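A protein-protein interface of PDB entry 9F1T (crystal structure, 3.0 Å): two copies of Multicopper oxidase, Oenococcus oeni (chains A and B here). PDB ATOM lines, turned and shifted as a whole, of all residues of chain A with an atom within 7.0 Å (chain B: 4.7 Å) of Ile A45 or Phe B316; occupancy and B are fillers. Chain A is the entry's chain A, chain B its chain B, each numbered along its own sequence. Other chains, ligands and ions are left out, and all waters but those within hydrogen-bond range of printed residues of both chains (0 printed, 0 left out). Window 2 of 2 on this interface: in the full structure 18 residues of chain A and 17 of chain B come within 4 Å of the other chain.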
ATOM      1  N   ALA A  42      31.107  13.783 -14.945  1.00  0.00           N
ATOM      2  CA  ALA A  42      31.942  13.080 -13.989  1.00  0.00           C
ATOM      3  C   ALA A  42      32.814  12.071 -14.725  1.00  0.00           C
ATOM      4  O   ALA A  42      32.330  11.369 -15.613  1.00  0.00           O
ATOM      5  CB  ALA A  42      31.077  12.402 -12.955  1.00  0.00           C
ATOM      6  N   ASP A  43      34.095  12.018 -14.342  1.00  0.00           N
ATOM      7  CA  ASP A  43      35.022  11.030 -14.863  1.00  0.00           C
ATOM      8  C   ASP A  43      34.533   9.638 -14.461  1.00  0.00           C
ATOM      9  O   ASP A  43      34.492   8.742 -15.301  1.00  0.00           O
ATOM     10  CB  ASP A  43      36.450  11.329 -14.425  1.00  0.00           C
ATOM     11  CG  ASP A  43      37.022  12.671 -14.878  1.00  0.00           C
ATOM     12  OD1 ASP A  43      36.241  13.528 -15.355  1.00  0.00           O
ATOM     13  OD2 ASP A  43      38.251  12.849 -14.764  1.00  0.00           O
ATOM     14  N   LYS A  44      34.143   9.484 -13.185  1.00  0.00           N
ATOM     15  CA  LYS A  44      33.598   8.236 -12.666  1.00  0.00           C
ATOM     16  C   LYS A  44      33.001   8.443 -11.275  1.00  0.00           C
ATOM     17  O   LYS A  44      33.343   9.395 -10.575  1.00  0.00           O
ATOM     18  CB  LYS A  44      34.669   7.143 -12.570  1.00  0.00           C
ATOM     19  CG  LYS A  44      35.907   7.474 -11.737  1.00  0.00           C
ATOM     20  CD  LYS A  44      37.025   6.455 -11.959  1.00  0.00           C
ATOM     21  CE  LYS A  44      38.329   6.774 -11.291  1.00  0.00           C
ATOM     22  NZ  LYS A  44      38.280   6.392  -9.879  1.00  0.00           N
ATOM     23  N   ILE A  45      32.103   7.524 -10.894  1.00  0.00           N
ATOM     24  CA  ILE A  45      31.567   7.446  -9.544  1.00  0.00           C
ATOM     25  C   ILE A  45      31.978   6.109  -8.939  1.00  0.00           C
ATOM     26  O   ILE A  45      31.736   5.059  -9.529  1.00  0.00           O
ATOM     27  CB  ILE A  45      30.036   7.593  -9.532  1.00  0.00           C
ATOM     28  CG1 ILE A  45      29.586   8.989  -9.969  1.00  0.00           C
ATOM     29  CG2 ILE A  45      29.476   7.222  -8.160  1.00  0.00           C
ATOM     30  CD1 ILE A  45      29.538   9.181 -11.475  1.00  0.00           C
ATOM     31  N   GLU A  46      32.581   6.165  -7.747  1.00  0.00           N
ATOM     32  CA  GLU A  46      33.134   4.991  -7.091  1.00  0.00           C
ATOM     33  C   GLU A  46      32.972   5.169  -5.584  1.00  0.00           C
ATOM     34  O   GLU A  46      33.708   5.936  -4.972  1.00  0.00           O
ATOM     35  CB  GLU A  46      34.578   4.860  -7.576  1.00  0.00           C
ATOM     36  CG  GLU A  46      35.343   3.652  -7.043  1.00  0.00           C
ATOM     37  CD  GLU A  46      36.687   3.438  -7.734  1.00  0.00           C
ATOM     38  OE1 GLU A  46      37.051   2.264  -7.992  1.00  0.00           O
ATOM     39  OE2 GLU A  46      37.373   4.448  -8.033  1.00  0.00           O
ATOM     40  N   GLY A  47      31.995   4.460  -5.004  1.00  0.00           N
ATOM     41  CA  GLY A  47      31.566   4.696  -3.634  1.00  0.00           C
ATOM     42  C   GLY A  47      30.726   5.969  -3.532  1.00  0.00           C
ATOM     43  O   GLY A  47      29.946   6.276  -4.434  1.00  0.00           O
ATOM     44  N   ASN A  48      30.902   6.710  -2.427  1.00  0.00           N
ATOM     45  CA  ASN A  48      30.250   8.000  -2.249  1.00  0.00           C
ATOM     46  C   ASN A  48      31.074   9.109  -2.910  1.00  0.00           C
ATOM     47  O   ASN A  48      30.699  10.281  -2.850  1.00  0.00           O
ATOM     48  CB  ASN A  48      30.019   8.267  -0.772  1.00  0.00           C
ATOM     49  N   THR A  49      32.185   8.727  -3.560  1.00  0.00           N
ATOM     50  CA  THR A  49      33.105   9.668  -4.178  1.00  0.00           C
ATOM     51  C   THR A  49      32.713   9.902  -5.636  1.00  0.00           C
ATOM     52  O   THR A  49      32.343   8.966  -6.342  1.00  0.00           O
ATOM     53  CB  THR A  49      34.523   9.111  -4.059  1.00  0.00           C
ATOM     54  OG1 THR A  49      34.729   9.023  -2.655  1.00  0.00           O
ATOM     55  CG2 THR A  49      35.578  10.018  -4.668  1.00  0.00           C
ATOM     56  N   THR A  50      32.838  11.161  -6.081  1.00  0.00           N
ATOM     57  CA  THR A  50      32.616  11.530  -7.472  1.00  0.00           C
ATOM     58  C   THR A  50      33.860  12.243  -8.011  1.00  0.00           C
ATOM     59  O   THR A  50      34.357  13.175  -7.382  1.00  0.00           O
ATOM     60  CB  THR A  50      31.360  12.399  -7.569  1.00  0.00           C
ATOM     61  OG1 THR A  50      30.254  11.644  -7.074  1.00  0.00           O
ATOM     62  CG2 THR A  50      31.069  12.839  -8.993  1.00  0.00           C
ATOM     63  N   TYR A  51      34.342  11.801  -9.185  1.00  0.00           N
ATOM     64  CA  TYR A  51      35.618  12.240  -9.735  1.00  0.00           C
ATOM     65  C   TYR A  51      35.418  13.267 -10.849  1.00  0.00           C
ATOM     66  O   TYR A  51      34.820  12.966 -11.878  1.00  0.00           O
ATOM     67  CB  TYR A  51      36.387  11.035 -10.283  1.00  0.00           C
ATOM     68  CG  TYR A  51      36.965  10.136  -9.202  1.00  0.00           C
ATOM     69  CD1 TYR A  51      36.162   9.244  -8.502  1.00  0.00           C
ATOM     70  CD2 TYR A  51      38.315  10.182  -8.882  1.00  0.00           C
ATOM     71  CE1 TYR A  51      36.684   8.425  -7.514  1.00  0.00           C
ATOM     72  CE2 TYR A  51      38.849   9.374  -7.891  1.00  0.00           C
ATOM     73  CZ  TYR A  51      38.031   8.491  -7.208  1.00  0.00           C
ATOM     74  OH  TYR A  51      38.566   7.685  -6.243  1.00  0.00           O
ATOM     75  N   ARG A  89      28.193  14.162   0.067  1.00  0.00           N
ATOM     76  CA  ARG A  89      28.964  13.353  -0.862  1.00  0.00           C
ATOM     77  C   ARG A  89      30.434  13.754  -0.777  1.00  0.00           C
ATOM     78  O   ARG A  89      30.752  14.886  -0.412  1.00  0.00           O
ATOM     79  CB  ARG A  89      28.463  13.488  -2.303  1.00  0.00           C
ATOM     80  CG  ARG A  89      27.131  12.805  -2.574  1.00  0.00           C
ATOM     81  CD  ARG A  89      26.908  12.543  -4.064  1.00  0.00           C
ATOM     82  NE  ARG A  89      27.811  11.493  -4.557  1.00  0.00           N
ATOM     83  CZ  ARG A  89      27.445  10.348  -5.131  1.00  0.00           C
ATOM     84  NH1 ARG A  89      26.176  10.126  -5.444  1.00  0.00           N
ATOM     85  NH2 ARG A  89      28.362   9.429  -5.397  1.00  0.00           N
ATOM     86  N   VAL B 229      19.416   0.538 -11.560  1.00  0.00           N
ATOM     87  CA  VAL B 229      19.019   1.687 -10.766  1.00  0.00           C
ATOM     88  C   VAL B 229      20.248   2.547 -10.487  1.00  0.00           C
ATOM     89  O   VAL B 229      21.266   2.047 -10.025  1.00  0.00           O
ATOM     90  CB  VAL B 229      18.356   1.217  -9.463  1.00  0.00           C
ATOM     91  CG1 VAL B 229      17.881   2.389  -8.612  1.00  0.00           C
ATOM     92  CG2 VAL B 229      17.208   0.254  -9.740  1.00  0.00           C
ATOM     93  N   THR B 230      20.144   3.844 -10.787  1.00  0.00           N
ATOM     94  CA  THR B 230      21.231   4.781 -10.563  1.00  0.00           C
ATOM     95  C   THR B 230      20.813   5.879  -9.582  1.00  0.00           C
ATOM     96  O   THR B 230      21.512   6.879  -9.443  1.00  0.00           O
ATOM     97  CB  THR B 230      21.666   5.353 -11.900  1.00  0.00           C
ATOM     98  N   ARG B 231      19.672   5.703  -8.900  1.00  0.00           N
ATOM     99  CA  ARG B 231      19.198   6.677  -7.926  1.00  0.00           C
ATOM    100  C   ARG B 231      18.435   5.962  -6.805  1.00  0.00           C
ATOM    101  O   ARG B 231      17.761   4.963  -7.043  1.00  0.00           O
ATOM    102  CB  ARG B 231      18.352   7.779  -8.579  1.00  0.00           C
ATOM    103  CG  ARG B 231      19.133   8.718  -9.488  1.00  0.00           C
ATOM    104  CD  ARG B 231      18.518  10.109  -9.638  1.00  0.00           C
ATOM    105  NE  ARG B 231      17.846  10.412 -10.910  1.00  0.00           N
ATOM    106  CZ  ARG B 231      18.175  11.400 -11.739  1.00  0.00           C
ATOM    107  NH1 ARG B 231      19.265  12.116 -11.551  1.00  0.00           N
ATOM    108  NH2 ARG B 231      17.420  11.671 -12.784  1.00  0.00           N
ATOM    109  N   PRO B 232      18.517   6.465  -5.550  1.00  0.00           N
ATOM    110  CA  PRO B 232      17.917   5.792  -4.392  1.00  0.00           C
ATOM    111  C   PRO B 232      16.415   5.517  -4.475  1.00  0.00           C
ATOM    112  O   PRO B 232      15.940   4.474  -4.030  1.00  0.00           O
ATOM    113  CB  PRO B 232      18.224   6.755  -3.230  1.00  0.00           C
ATOM    114  CG  PRO B 232      19.424   7.543  -3.685  1.00  0.00           C
ATOM    115  CD  PRO B 232      19.231   7.699  -5.179  1.00  0.00           C
ATOM    116  N   PHE B 290      16.180   2.328  -2.255  1.00  0.00           N
ATOM    117  CA  PHE B 290      17.317   1.432  -2.368  1.00  0.00           C
ATOM    118  C   PHE B 290      18.472   1.907  -1.488  1.00  0.00           C
ATOM    119  O   PHE B 290      19.591   1.430  -1.646  1.00  0.00           O
ATOM    120  CB  PHE B 290      17.708   1.357  -3.845  1.00  0.00           C
ATOM    121  CG  PHE B 290      16.686   0.682  -4.751  1.00  0.00           C
ATOM    122  CD1 PHE B 290      16.729  -0.688  -4.971  1.00  0.00           C
ATOM    123  CD2 PHE B 290      15.705   1.421  -5.406  1.00  0.00           C
ATOM    124  CE1 PHE B 290      15.811  -1.301  -5.809  1.00  0.00           C
ATOM    125  CE2 PHE B 290      14.788   0.801  -6.240  1.00  0.00           C
ATOM    126  CZ  PHE B 290      14.840  -0.558  -6.433  1.00  0.00           C
ATOM    127  N   VAL B 313      21.328  -2.844  -8.750  1.00  0.00           N
ATOM    128  CA  VAL B 313      21.735  -1.596  -8.129  1.00  0.00           C
ATOM    129  C   VAL B 313      23.124  -1.212  -8.623  1.00  0.00           C
ATOM    130  O   VAL B 313      24.080  -1.951  -8.410  1.00  0.00           O
ATOM    131  CB  VAL B 313      21.718  -1.713  -6.596  1.00  0.00           C
ATOM    132  CG1 VAL B 313      22.113  -0.400  -5.922  1.00  0.00           C
ATOM    133  CG2 VAL B 313      20.362  -2.196  -6.096  1.00  0.00           C
ATOM    134  N   GLY B 314      23.209  -0.043  -9.272  1.00  0.00           N
ATOM    135  CA  GLY B 314      24.470   0.524  -9.720  1.00  0.00           C
ATOM    136  C   GLY B 314      24.966   1.595  -8.750  1.00  0.00           C
ATOM    137  O   GLY B 314      24.432   1.729  -7.648  1.00  0.00           O
ATOM    138  N   GLU B 315      26.000   2.336  -9.172  1.00  0.00           N
ATOM    139  CA  GLU B 315      26.468   3.496  -8.433  1.00  0.00           C
ATOM    140  C   GLU B 315      25.441   4.611  -8.597  1.00  0.00           C
ATOM    141  O   GLU B 315      25.027   4.905  -9.715  1.00  0.00           O
ATOM    142  CB  GLU B 315      27.838   3.970  -8.922  1.00  0.00           C
ATOM    143  CG  GLU B 315      28.978   3.026  -8.549  1.00  0.00           C
ATOM    144  CD  GLU B 315      29.481   3.134  -7.120  1.00  0.00           C
ATOM    145  OE1 GLU B 315      28.665   3.421  -6.211  1.00  0.00           O
ATOM    146  OE2 GLU B 315      30.696   2.885  -6.922  1.00  0.00           O
ATOM    147  N   PHE B 316      25.028   5.207  -7.474  1.00  0.00           N
ATOM    148  CA  PHE B 316      24.027   6.257  -7.493  1.00  0.00           C
ATOM    149  C   PHE B 316      24.687   7.576  -7.877  1.00  0.00           C
ATOM    150  O   PHE B 316      25.784   7.877  -7.418  1.00  0.00           O
ATOM    151  CB  PHE B 316      23.319   6.397  -6.143  1.00  0.00           C
ATOM    152  CG  PHE B 316      22.474   5.211  -5.698  1.00  0.00           C
ATOM    153  CD1 PHE B 316      22.015   4.259  -6.608  1.00  0.00           C
ATOM    154  CD2 PHE B 316      22.117   5.071  -4.358  1.00  0.00           C
ATOM    155  CE1 PHE B 316      21.243   3.188  -6.178  1.00  0.00           C
ATOM    156  CE2 PHE B 316      21.342   4.000  -3.937  1.00  0.00           C
ATOM    157  CZ  PHE B 316      20.908   3.061  -4.847  1.00  0.00           C
ATOM    158  N   THR B 317      23.993   8.355  -8.715  1.00  0.00           N
ATOM    159  CA  THR B 317      24.499   9.630  -9.194  1.00  0.00           C
ATOM    160  C   THR B 317      24.092  10.722  -8.207  1.00  0.00           C
ATOM    161  O   THR B 317      24.944  11.502  -7.785  1.00  0.00           O
ATOM    162  CB  THR B 317      23.999   9.908 -10.614  1.00  0.00           C
ATOM    163  OG1 THR B 317      22.590  10.117 -10.577  1.00  0.00           O
ATOM    164  CG2 THR B 317      24.323   8.772 -11.569  1.00  0.00           C
ATOM    165  N   GLU B 318      22.800  10.755  -7.840  1.00  0.00           N
ATOM    166  CA  GLU B 318      22.256  11.753  -6.932  1.00  0.00           C
ATOM    167  C   GLU B 318      21.532  11.064  -5.780  1.00  0.00           C
ATOM    168  O   GLU B 318      21.417   9.840  -5.766  1.00  0.00           O
ATOM    169  CB  GLU B 318      21.177  12.615  -7.591  1.00  0.00           C
ATOM    170  CG  GLU B 318      21.548  13.236  -8.935  1.00  0.00           C
ATOM    171  CD  GLU B 318      20.423  14.085  -9.514  1.00  0.00           C
ATOM    172  OE1 GLU B 318      20.630  14.758 -10.554  1.00  0.00           O
ATOM    173  OE2 GLU B 318      19.317  14.049  -8.924  1.00  0.00           O
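The side-chain hydroxyl (OG1) of Thr A50 sits at hydrogen-bond distance from the guanidinium group (NH2) of Arg A89, 3.4 Å away.
The backbone carbonyl oxygen of Thr B230 lies within hydrogen-bond range of the backbone NH of Thr B317, 3.0 Å away.
NZ of Lys A44 lies within salt-bridge range of OE2 of Glu A46, at 2.8 Å.
Ile A45 touches Glu B315 (O to OE2, 3.6 Å).
O of Phe B316 touches CG2 of Ile A45, 3.8 Å away.
Glu B315 touches Glu A46 (OE2 to CA, 3.2 Å).
No position is printed for both chains.
Of the 6 pairs that touch across the chains among the printed residues, none has its exchanged pair printed and touching as well.
Ile A45 touches just these residues of chain B: Glu B315 and Phe B316.
Phe B316 touches just these residues of chain A: Ile A45 (3.8 Å) and Arg A89 (3.0 Å).
Printed residues of chain B within 4 Å of Glu A46: Glu B315 (3.2 Å).
Printed residues of chain A within 4 Å of Glu B315: Ile A45, Glu A46 and Gly A47.
Of the printed residues of chain B, Arg A89 touches Phe B316 and Thr B317.
Printed residues of chain A within 4 Å of Thr B317: Arg A89.
Lys A44 touches none of the printed residues of chain B.
The nearest residue of chain A that does not touch Phe B316 is Gly A47 (5.4 Å).
Of the 11 printed residues of chain B, 3 touch a printed residue of chain A.
Hydrophobic or aromatic side chains of chain A within 4 Å of the printed part of chain B: Ile A45.
O of Thr B317 sits at hydrogen-bond distance from NH1 of Arg A89 (3.0 Å).
The backbone carbonyl oxygen of Phe B316 lies within hydrogen-bond range of the guanidinium group of Arg A89 (3.0 Å).
The side-chain carboxylate (OE2) of Glu B315 is in hydrogen-bond range of the backbone NH (N) of Gly A47 (2.8 Å).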
